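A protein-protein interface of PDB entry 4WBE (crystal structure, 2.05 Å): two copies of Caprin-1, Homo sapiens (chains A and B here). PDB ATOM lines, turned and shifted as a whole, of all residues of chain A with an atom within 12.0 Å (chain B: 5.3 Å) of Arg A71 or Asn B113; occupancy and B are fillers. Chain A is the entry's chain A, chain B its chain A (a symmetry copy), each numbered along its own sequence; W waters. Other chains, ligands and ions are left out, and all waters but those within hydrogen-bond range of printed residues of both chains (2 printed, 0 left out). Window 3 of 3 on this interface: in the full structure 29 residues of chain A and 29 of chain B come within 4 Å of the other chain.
Arg A71 touches two residues of chain B. Asn B113 touches just one residue of chain A: Arg A71. Phe B115 touches two residues of chain A. Printed residues of chain A within 4 Å of Asp B116: Arg A66 (3.5 Å), Arg A71 (2.8 Å) and Leu A72 (2.9 Å). Ser B117 touches none of the printed residues of chain A. Of the printed residues of chain B, Leu A72 touches Phe B110, Phe B115 and Asp B116. Of the printed residues of chain A, Phe B110 touches Leu A72. Val B109 touches none of the printed residues of chain A. Gln B111 touches none of the printed residues of chain A. The nearest printed residue of chain B that does not touch Arg A66 is Ser B117 (4.7 Å).
The side-chain carboxylate (OD2) of Asp B116 lies within salt-bridge range of the guanidinium group (NE) of Arg A71. The backbone NH of Leu A72 lies within hydrogen-bond range of the side-chain carboxylate of Asp B116 (2.9 Å). NH2 of Arg A71 lies within hydrogen-bond range of OD1 of Asn B113 (3.1 Å). The backbone carbonyl oxygen (O) of Phe B115 lies within hydrogen-bond range of the guanidinium group (NH2) of Arg A66, at 3.0 Å.
Of the 9 printed residues of chain B, 4 touch a printed residue of chain A. Printed residues of chain B that touch a printed residue of chain A: Phe B110, Asn B113, Phe B115 and Asp B116. Hydrophobic or aromatic side chains of chain B that line the printed part of chain A: Phe B110 and Phe B115. Hydrophobic or aromatic side chains of chain A that line the printed part of chain B: Leu A72. Along chain A the printed residues that touch a printed residue of chain B span positions 66 to 72.
Water W2 lies within hydrogen-bond range of the side-chain amide nitrogen of Asn A73 (2.6 Å), the side-chain carboxylate of Asp B116 (2.7 Å) and the backbone NH of Leu A72 (3.3 Å). Water W1 lies within hydrogen-bond range of O of Phe B115 (2.8 Å), NE of Arg A66 (2.9 Å) and O of Ser B117 (3.0 Å).
No position is printed for both chains. Of the 7 pairs that touch across the chains among the printed residues, none has its exchanged pair printed and touching as well.
Among the printed residues, merely in contact across the chains: Arg A66 with Asp B116, Leu A72 with Phe B110 and Leu A72 with Phe B115.
The side-chain carboxylate (OE1) of Glu A74 lies within hydrogen-bond range of the backbone NH (N) of Arg A71 (3.0 Å). The side-chain amide oxygen (OD1) of Asn B113 sits close to the backbone carbonyl oxygen (O) of Phe B110, at 3.5 Å. OD2 of Asp B116 sits close to OD1 of Asn B113 (3.3 Å). The side-chain amide oxygen (OE1) of Gln A75 is in hydrogen-bond range of the guanidinium group (NH1) of Arg A66 (3.0 Å). The guanidinium group (NH1) of Arg A66 sits at hydrogen-bond distance from the backbone carbonyl oxygen (O) of Leu A70, at 2.8 Å.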
ATOM      1  N   PRO A  64     -19.985  -9.900  33.623  1.00  0.00           N
ATOM      2  CA  PRO A  64     -18.594 -10.362  33.670  1.00  0.00           C
ATOM      3  C   PRO A  64     -17.623  -9.266  34.075  1.00  0.00           C
ATOM      4  O   PRO A  64     -17.848  -8.090  33.778  1.00  0.00           O
ATOM      5  CB  PRO A  64     -18.321 -10.802  32.222  1.00  0.00           C
ATOM      6  CG  PRO A  64     -19.273  -9.993  31.385  1.00  0.00           C
ATOM      7  CD  PRO A  64     -20.508  -9.838  32.244  1.00  0.00           C
ATOM      8  N   GLU A  65     -16.565  -9.654  34.775  1.00  0.00           N
ATOM      9  CA  GLU A  65     -15.468  -8.740  35.022  1.00  0.00           C
ATOM     10  C   GLU A  65     -14.817  -8.401  33.696  1.00  0.00           C
ATOM     11  O   GLU A  65     -14.806  -9.213  32.767  1.00  0.00           O
ATOM     12  CB  GLU A  65     -14.428  -9.346  35.969  1.00  0.00           C
ATOM     13  CG  GLU A  65     -14.931  -9.614  37.380  1.00  0.00           C
ATOM     14  CD  GLU A  65     -15.350  -8.352  38.125  1.00  0.00           C
ATOM     15  OE1 GLU A  65     -15.155  -7.229  37.609  1.00  0.00           O
ATOM     16  OE2 GLU A  65     -15.878  -8.490  39.249  1.00  0.00           O
ATOM     17  N   ARG A  66     -14.282  -7.192  33.619  1.00  0.00           N
ATOM     18  CA  ARG A  66     -13.669  -6.690  32.404  1.00  0.00           C
ATOM     19  C   ARG A  66     -12.422  -7.517  32.066  1.00  0.00           C
ATOM     20  O   ARG A  66     -11.491  -7.604  32.866  1.00  0.00           O
ATOM     21  CB  ARG A  66     -13.319  -5.219  32.606  1.00  0.00           C
ATOM     22  CG  ARG A  66     -12.885  -4.513  31.358  1.00  0.00           C
ATOM     23  CD  ARG A  66     -14.030  -4.336  30.373  1.00  0.00           C
ATOM     24  NE  ARG A  66     -13.536  -3.670  29.174  1.00  0.00           N
ATOM     25  CZ  ARG A  66     -13.042  -4.306  28.119  1.00  0.00           C
ATOM     26  NH1 ARG A  66     -13.006  -5.633  28.096  1.00  0.00           N
ATOM     27  NH2 ARG A  66     -12.595  -3.616  27.077  1.00  0.00           N
ATOM     28  N   ASP A  67     -12.428  -8.141  30.889  1.00  0.00           N
ATOM     29  CA  ASP A  67     -11.321  -8.978  30.419  1.00  0.00           C
ATOM     30  C   ASP A  67     -10.443  -8.203  29.425  1.00  0.00           C
ATOM     31  O   ASP A  67     -10.911  -7.805  28.355  1.00  0.00           O
ATOM     32  CB  ASP A  67     -11.893 -10.258  29.786  1.00  0.00           C
ATOM     33  CG  ASP A  67     -10.820 -11.276  29.398  1.00  0.00           C
ATOM     34  OD1 ASP A  67      -9.633 -10.910  29.246  1.00  0.00           O
ATOM     35  OD2 ASP A  67     -11.181 -12.465  29.241  1.00  0.00           O
ATOM     36  N   MET A  68      -9.172  -8.010  29.776  1.00  0.00           N
ATOM     37  CA  MET A  68      -8.268  -7.164  28.987  1.00  0.00           C
ATOM     38  C   MET A  68      -7.966  -7.696  27.579  1.00  0.00           C
ATOM     39  O   MET A  68      -7.495  -6.950  26.717  1.00  0.00           O
ATOM     40  CB  MET A  68      -6.973  -6.892  29.783  1.00  0.00           C
ATOM     41  CG  MET A  68      -5.841  -7.933  29.636  1.00  0.00           C
ATOM     42  SD  MET A  68      -4.323  -7.508  30.569  1.00  0.00           S
ATOM     43  CE  MET A  68      -4.949  -7.669  32.223  1.00  0.00           C
ATOM     44  N   SER A  69      -8.251  -8.973  27.338  1.00  0.00           N
ATOM     45  CA  SER A  69      -8.091  -9.545  26.005  1.00  0.00           C
ATOM     46  C   SER A  69      -9.297  -9.241  25.110  1.00  0.00           C
ATOM     47  O   SER A  69      -9.283  -9.549  23.918  1.00  0.00           O
ATOM     48  CB  SER A  69      -7.892 -11.058  26.095  1.00  0.00           C
ATOM     49  OG  SER A  69      -9.089 -11.688  26.502  1.00  0.00           O
ATOM     50  N   LEU A  70     -10.331  -8.628  25.680  1.00  0.00           N
ATOM     51  CA  LEU A  70     -11.539  -8.304  24.922  1.00  0.00           C
ATOM     52  C   LEU A  70     -11.749  -6.803  24.767  1.00  0.00           C
ATOM     53  O   LEU A  70     -11.588  -6.038  25.718  1.00  0.00           O
ATOM     54  CB  LEU A  70     -12.785  -8.911  25.582  1.00  0.00           C
ATOM     55  CG  LEU A  70     -12.926 -10.431  25.651  1.00  0.00           C
ATOM     56  CD1 LEU A  70     -14.253 -10.825  26.307  1.00  0.00           C
ATOM     57  CD2 LEU A  70     -12.803 -11.043  24.257  1.00  0.00           C
ATOM     58  N   ARG A  71     -12.106  -6.387  23.558  1.00  0.00           N
ATOM     59  CA  ARG A  71     -12.521  -5.009  23.328  1.00  0.00           C
ATOM     60  C   ARG A  71     -13.892  -4.776  23.965  1.00  0.00           C
ATOM     61  O   ARG A  71     -14.600  -5.735  24.288  1.00  0.00           O
ATOM     62  CB  ARG A  71     -12.566  -4.711  21.827  1.00  0.00           C
ATOM     63  CG  ARG A  71     -11.202  -4.774  21.142  1.00  0.00           C
ATOM     64  CD  ARG A  71     -11.310  -4.395  19.674  1.00  0.00           C
ATOM     65  NE  ARG A  71     -11.745  -3.008  19.531  1.00  0.00           N
ATOM     66  CZ  ARG A  71     -12.098  -2.442  18.381  1.00  0.00           C
ATOM     67  NH1 ARG A  71     -12.085  -3.144  17.253  1.00  0.00           N
ATOM     68  NH2 ARG A  71     -12.473  -1.169  18.362  1.00  0.00           N
ATOM     69  N   LEU A  72     -14.264  -3.513  24.158  1.00  0.00           N
ATOM     70  CA  LEU A  72     -15.558  -3.188  24.762  1.00  0.00           C
ATOM     71  C   LEU A  72     -16.728  -3.779  23.971  1.00  0.00           C
ATOM     72  O   LEU A  72     -17.689  -4.302  24.558  1.00  0.00           O
ATOM     73  CB  LEU A  72     -15.744  -1.668  24.872  1.00  0.00           C
ATOM     74  CG  LEU A  72     -17.092  -1.197  25.441  1.00  0.00           C
ATOM     75  CD1 LEU A  72     -17.270  -1.638  26.894  1.00  0.00           C
ATOM     76  CD2 LEU A  72     -17.294   0.321  25.289  1.00  0.00           C
ATOM     77  N   ASN A  73     -16.645  -3.717  22.647  1.00  0.00           N
ATOM     78  CA  ASN A  73     -17.746  -4.191  21.800  1.00  0.00           C
ATOM     79  C   ASN A  73     -17.884  -5.714  21.810  1.00  0.00           C
ATOM     80  O   ASN A  73     -18.862  -6.259  21.291  1.00  0.00           O
ATOM     81  CB  ASN A  73     -17.554  -3.705  20.355  1.00  0.00           C
ATOM     82  CG  ASN A  73     -16.487  -4.480  19.611  1.00  0.00           C
ATOM     83  OD1 ASN A  73     -16.730  -5.598  19.146  1.00  0.00           O
ATOM     84  ND2 ASN A  73     -15.295  -3.914  19.518  1.00  0.00           N
ATOM     85  N   GLU A  74     -16.910  -6.396  22.408  1.00  0.00           N
ATOM     86  CA  GLU A  74     -16.939  -7.851  22.516  1.00  0.00           C
ATOM     87  C   GLU A  74     -17.282  -8.353  23.911  1.00  0.00           C
ATOM     88  O   GLU A  74     -17.778  -9.474  24.070  1.00  0.00           O
ATOM     89  CB  GLU A  74     -15.557  -8.403  22.167  1.00  0.00           C
ATOM     90  CG  GLU A  74     -15.094  -8.153  20.753  1.00  0.00           C
ATOM     91  CD  GLU A  74     -13.669  -8.633  20.526  1.00  0.00           C
ATOM     92  OE1 GLU A  74     -12.751  -8.194  21.257  1.00  0.00           O
ATOM     93  OE2 GLU A  74     -13.480  -9.497  19.653  1.00  0.00           O
ATOM     94  N   GLN A  75     -16.989  -7.532  24.913  1.00  0.00           N
ATOM     95  CA  GLN A  75     -17.098  -7.930  26.317  1.00  0.00           C
ATOM     96  C   GLN A  75     -18.453  -8.508  26.703  1.00  0.00           C
ATOM     97  O   GLN A  75     -18.540  -9.412  27.532  1.00  0.00           O
ATOM     98  CB  GLN A  75     -16.751  -6.750  27.226  1.00  0.00           C
ATOM     99  CG  GLN A  75     -16.849  -7.042  28.722  1.00  0.00           C
ATOM    100  CD  GLN A  75     -15.845  -8.093  29.168  1.00  0.00           C
ATOM    101  OE1 GLN A  75     -14.645  -7.823  29.267  1.00  0.00           O
ATOM    102  NE2 GLN A  75     -16.336  -9.295  29.466  1.00  0.00           N
ATOM    103  N   TYR A  76     -19.514  -7.982  26.108  1.00  0.00           N
ATOM    104  CA  TYR A  76     -20.858  -8.355  26.532  1.00  0.00           C
ATOM    105  C   TYR A  76     -21.653  -9.146  25.508  1.00  0.00           C
ATOM    106  O   TYR A  76     -22.876  -9.272  25.635  1.00  0.00           O
ATOM    107  CB  TYR A  76     -21.620  -7.106  26.964  1.00  0.00           C
ATOM    108  CG  TYR A  76     -21.027  -6.467  28.192  1.00  0.00           C
ATOM    109  CD1 TYR A  76     -21.269  -7.001  29.447  1.00  0.00           C
ATOM    110  CD2 TYR A  76     -20.234  -5.330  28.100  1.00  0.00           C
ATOM    111  CE1 TYR A  76     -20.739  -6.427  30.575  1.00  0.00           C
ATOM    112  CE2 TYR A  76     -19.696  -4.746  29.229  1.00  0.00           C
ATOM    113  CZ  TYR A  76     -19.953  -5.303  30.462  1.00  0.00           C
ATOM    114  OH  TYR A  76     -19.436  -4.746  31.601  1.00  0.00           O
ATOM    115  N   GLU A  77     -20.968  -9.684  24.502  1.00  0.00           N
ATOM    116  CA  GLU A  77     -21.639 -10.493  23.502  1.00  0.00           C
ATOM    117  C   GLU A  77     -22.292 -11.719  24.152  1.00  0.00           C
ATOM    118  O   GLU A  77     -23.501 -11.928  24.018  1.00  0.00           O
ATOM    119  CB  GLU A  77     -20.661 -10.897  22.387  1.00  0.00           C
ATOM    120  CG  GLU A  77     -21.243 -11.865  21.371  1.00  0.00           C
ATOM    121  CD  GLU A  77     -22.263 -11.207  20.443  1.00  0.00           C
ATOM    122  OE1 GLU A  77     -22.232  -9.965  20.287  1.00  0.00           O
ATOM    123  OE2 GLU A  77     -23.092 -11.939  19.861  1.00  0.00           O
ATOM    124  N   HIS A  78     -21.508 -12.509  24.882  1.00  0.00           N
ATOM    125  CA  HIS A  78     -22.049 -13.694  25.554  1.00  0.00           C
ATOM    126  C   HIS A  78     -23.126 -13.348  26.582  1.00  0.00           C
ATOM    127  O   HIS A  78     -24.172 -14.005  26.632  1.00  0.00           O
ATOM    128  CB  HIS A  78     -20.934 -14.503  26.227  1.00  0.00           C
ATOM    129  CG  HIS A  78     -20.072 -15.254  25.267  1.00  0.00           C
ATOM    130  ND1 HIS A  78     -20.423 -15.462  23.951  1.00  0.00           N
ATOM    131  CD2 HIS A  78     -18.863 -15.849  25.429  1.00  0.00           C
ATOM    132  CE1 HIS A  78     -19.474 -16.155  23.346  1.00  0.00           C
ATOM    133  NE2 HIS A  78     -18.518 -16.399  24.223  1.00  0.00           N
ATOM    134  N   ALA A  79     -22.864 -12.323  27.393  1.00  0.00           N
ATOM    135  CA  ALA A  79     -23.814 -11.876  28.406  1.00  0.00           C
ATOM    136  C   ALA A  79     -25.164 -11.516  27.799  1.00  0.00           C
ATOM    137  O   ALA A  79     -26.212 -11.816  28.379  1.00  0.00           O
ATOM    138  CB  ALA A  79     -23.250 -10.688  29.192  1.00  0.00           C
ATOM    139  N   SER A  80     -25.135 -10.833  26.656  1.00  0.00           N
ATOM    140  CA  SER A  80     -26.365 -10.428  25.973  1.00  0.00           C
ATOM    141  C   SER A  80     -27.210 -11.642  25.592  1.00  0.00           C
ATOM    142  O   SER A  80     -28.441 -11.622  25.704  1.00  0.00           O
ATOM    143  CB  SER A  80     -26.063  -9.554  24.744  1.00  0.00           C
ATOM    144  OG  SER A  80     -25.437 -10.283  23.705  1.00  0.00           O
ATOM    145  N   VAL B 109     -18.110   8.132  22.114  1.00  0.00           N
ATOM    146  CA  VAL B 109     -17.423   7.523  23.252  1.00  0.00           C
ATOM    147  C   VAL B 109     -17.045   6.065  22.963  1.00  0.00           C
ATOM    148  O   VAL B 109     -15.883   5.680  23.134  1.00  0.00           O
ATOM    149  CB  VAL B 109     -18.270   7.597  24.540  1.00  0.00           C
ATOM    150  CG1 VAL B 109     -17.581   6.850  25.670  1.00  0.00           C
ATOM    151  CG2 VAL B 109     -18.498   9.041  24.942  1.00  0.00           C
ATOM    152  N   PHE B 110     -18.017   5.274  22.509  1.00  0.00           N
ATOM    153  CA  PHE B 110     -17.771   3.894  22.097  1.00  0.00           C
ATOM    154  C   PHE B 110     -16.638   3.807  21.076  1.00  0.00           C
ATOM    155  O   PHE B 110     -15.726   2.987  21.203  1.00  0.00           O
ATOM    156  CB  PHE B 110     -19.025   3.302  21.439  1.00  0.00           C
ATOM    157  CG  PHE B 110     -20.096   2.869  22.407  1.00  0.00           C
ATOM    158  CD1 PHE B 110     -19.841   2.796  23.767  1.00  0.00           C
ATOM    159  CD2 PHE B 110     -21.360   2.520  21.945  1.00  0.00           C
ATOM    160  CE1 PHE B 110     -20.834   2.380  24.662  1.00  0.00           C
ATOM    161  CE2 PHE B 110     -22.358   2.101  22.833  1.00  0.00           C
ATOM    162  CZ  PHE B 110     -22.092   2.031  24.190  1.00  0.00           C
ATOM    163  N   GLN B 111     -16.713   4.658  20.059  1.00  0.00           N
ATOM    164  CA  GLN B 111     -15.828   4.564  18.905  1.00  0.00           C
ATOM    165  C   GLN B 111     -14.448   5.172  19.154  1.00  0.00           C
ATOM    166  O   GLN B 111     -13.537   5.021  18.348  1.00  0.00           O
ATOM    167  CB  GLN B 111     -16.517   5.143  17.661  1.00  0.00           C
ATOM    168  CG  GLN B 111     -17.695   4.265  17.191  1.00  0.00           C
ATOM    169  CD  GLN B 111     -18.543   4.903  16.102  1.00  0.00           C
ATOM    170  OE1 GLN B 111     -18.084   5.776  15.370  1.00  0.00           O
ATOM    171  NE2 GLN B 111     -19.796   4.476  16.003  1.00  0.00           N
ATOM    172  N   SER B 112     -14.294   5.863  20.275  1.00  0.00           N
ATOM    173  CA  SER B 112     -13.004   6.431  20.633  1.00  0.00           C
ATOM    174  C   SER B 112     -12.034   5.317  21.004  1.00  0.00           C
ATOM    175  O   SER B 112     -10.817   5.494  20.958  1.00  0.00           O
ATOM    176  CB  SER B 112     -13.167   7.367  21.825  1.00  0.00           C
ATOM    177  OG  SER B 112     -13.278   6.621  23.019  1.00  0.00           O
ATOM    178  N   ASN B 113     -12.604   4.177  21.391  1.00  0.00           N
ATOM    179  CA  ASN B 113     -11.864   3.015  21.876  1.00  0.00           C
ATOM    180  C   ASN B 113     -11.098   3.226  23.181  1.00  0.00           C
ATOM    181  O   ASN B 113     -10.229   2.429  23.531  1.00  0.00           O
ATOM    182  CB  ASN B 113     -10.990   2.408  20.780  1.00  0.00           C
ATOM    183  CG  ASN B 113     -11.807   1.966  19.590  1.00  0.00           C
ATOM    184  OD1 ASN B 113     -12.959   1.522  19.736  1.00  0.00           O
ATOM    185  ND2 ASN B 113     -11.228   2.079  18.409  1.00  0.00           N
ATOM    186  N   TYR B 114     -11.424   4.303  23.891  1.00  0.00           N
ATOM    187  CA  TYR B 114     -10.842   4.557  25.207  1.00  0.00           C
ATOM    188  C   TYR B 114     -11.076   3.360  26.122  1.00  0.00           C
ATOM    189  O   TYR B 114     -10.176   2.918  26.841  1.00  0.00           O
ATOM    190  CB  TYR B 114     -11.461   5.815  25.832  1.00  0.00           C
ATOM    191  CG  TYR B 114     -11.009   6.080  27.254  1.00  0.00           C
ATOM    192  CD1 TYR B 114      -9.807   6.733  27.506  1.00  0.00           C
ATOM    193  CD2 TYR B 114     -11.788   5.699  28.338  1.00  0.00           C
ATOM    194  CE1 TYR B 114      -9.381   6.980  28.799  1.00  0.00           C
ATOM    195  CE2 TYR B 114     -11.372   5.944  29.642  1.00  0.00           C
ATOM    196  CZ  TYR B 114     -10.167   6.590  29.864  1.00  0.00           C
ATOM    197  OH  TYR B 114      -9.750   6.833  31.153  1.00  0.00           O
ATOM    198  N   PHE B 115     -12.292   2.821  26.061  1.00  0.00           N
ATOM    199  CA  PHE B 115     -12.705   1.747  26.952  1.00  0.00           C
ATOM    200  C   PHE B 115     -12.303   0.349  26.479  1.00  0.00           C
ATOM    201  O   PHE B 115     -12.703  -0.650  27.081  1.00  0.00           O
ATOM    202  CB  PHE B 115     -14.210   1.833  27.243  1.00  0.00           C
ATOM    203  CG  PHE B 115     -14.588   3.027  28.069  1.00  0.00           C
ATOM    204  CD1 PHE B 115     -14.305   3.060  29.430  1.00  0.00           C
ATOM    205  CD2 PHE B 115     -15.225   4.115  27.493  1.00  0.00           C
ATOM    206  CE1 PHE B 115     -14.645   4.162  30.201  1.00  0.00           C
ATOM    207  CE2 PHE B 115     -15.572   5.221  28.253  1.00  0.00           C
ATOM    208  CZ  PHE B 115     -15.283   5.246  29.611  1.00  0.00           C
ATOM    209  N   ASP B 116     -11.519   0.280  25.403  1.00  0.00           N
ATOM    210  CA  ASP B 116     -10.946  -0.988  24.963  1.00  0.00           C
ATOM    211  C   ASP B 116      -9.785  -1.394  25.871  1.00  0.00           C
ATOM    212  O   ASP B 116      -9.412  -2.565  25.925  1.00  0.00           O
ATOM    213  CB  ASP B 116     -10.489  -0.929  23.505  1.00  0.00           C
ATOM    214  CG  ASP B 116     -11.639  -1.041  22.525  1.00  0.00           C
ATOM    215  OD1 ASP B 116     -12.787  -1.293  22.956  1.00  0.00           O
ATOM    216  OD2 ASP B 116     -11.387  -0.889  21.314  1.00  0.00           O
ATOM    217  N   SER B 117      -9.211  -0.433  26.587  1.00  0.00           N
ATOM    218  CA  SER B 117      -8.222  -0.787  27.587  1.00  0.00           C
ATOM    219  C   SER B 117      -8.926  -0.756  28.935  1.00  0.00           C
ATOM    220  O   SER B 117      -9.930  -0.057  29.103  1.00  0.00           O
ATOM    221  CB  SER B 117      -7.065   0.216  27.594  1.00  0.00           C
ATOM    222  OG  SER B 117      -6.643   0.556  26.286  1.00  0.00           O
HETATM  223  O   HOH W   1     -12.626  -1.062  29.880  1.00  0.00           O
HETATM  224  O   HOH W   2     -14.795  -2.008  21.262  1.00  0.00           O
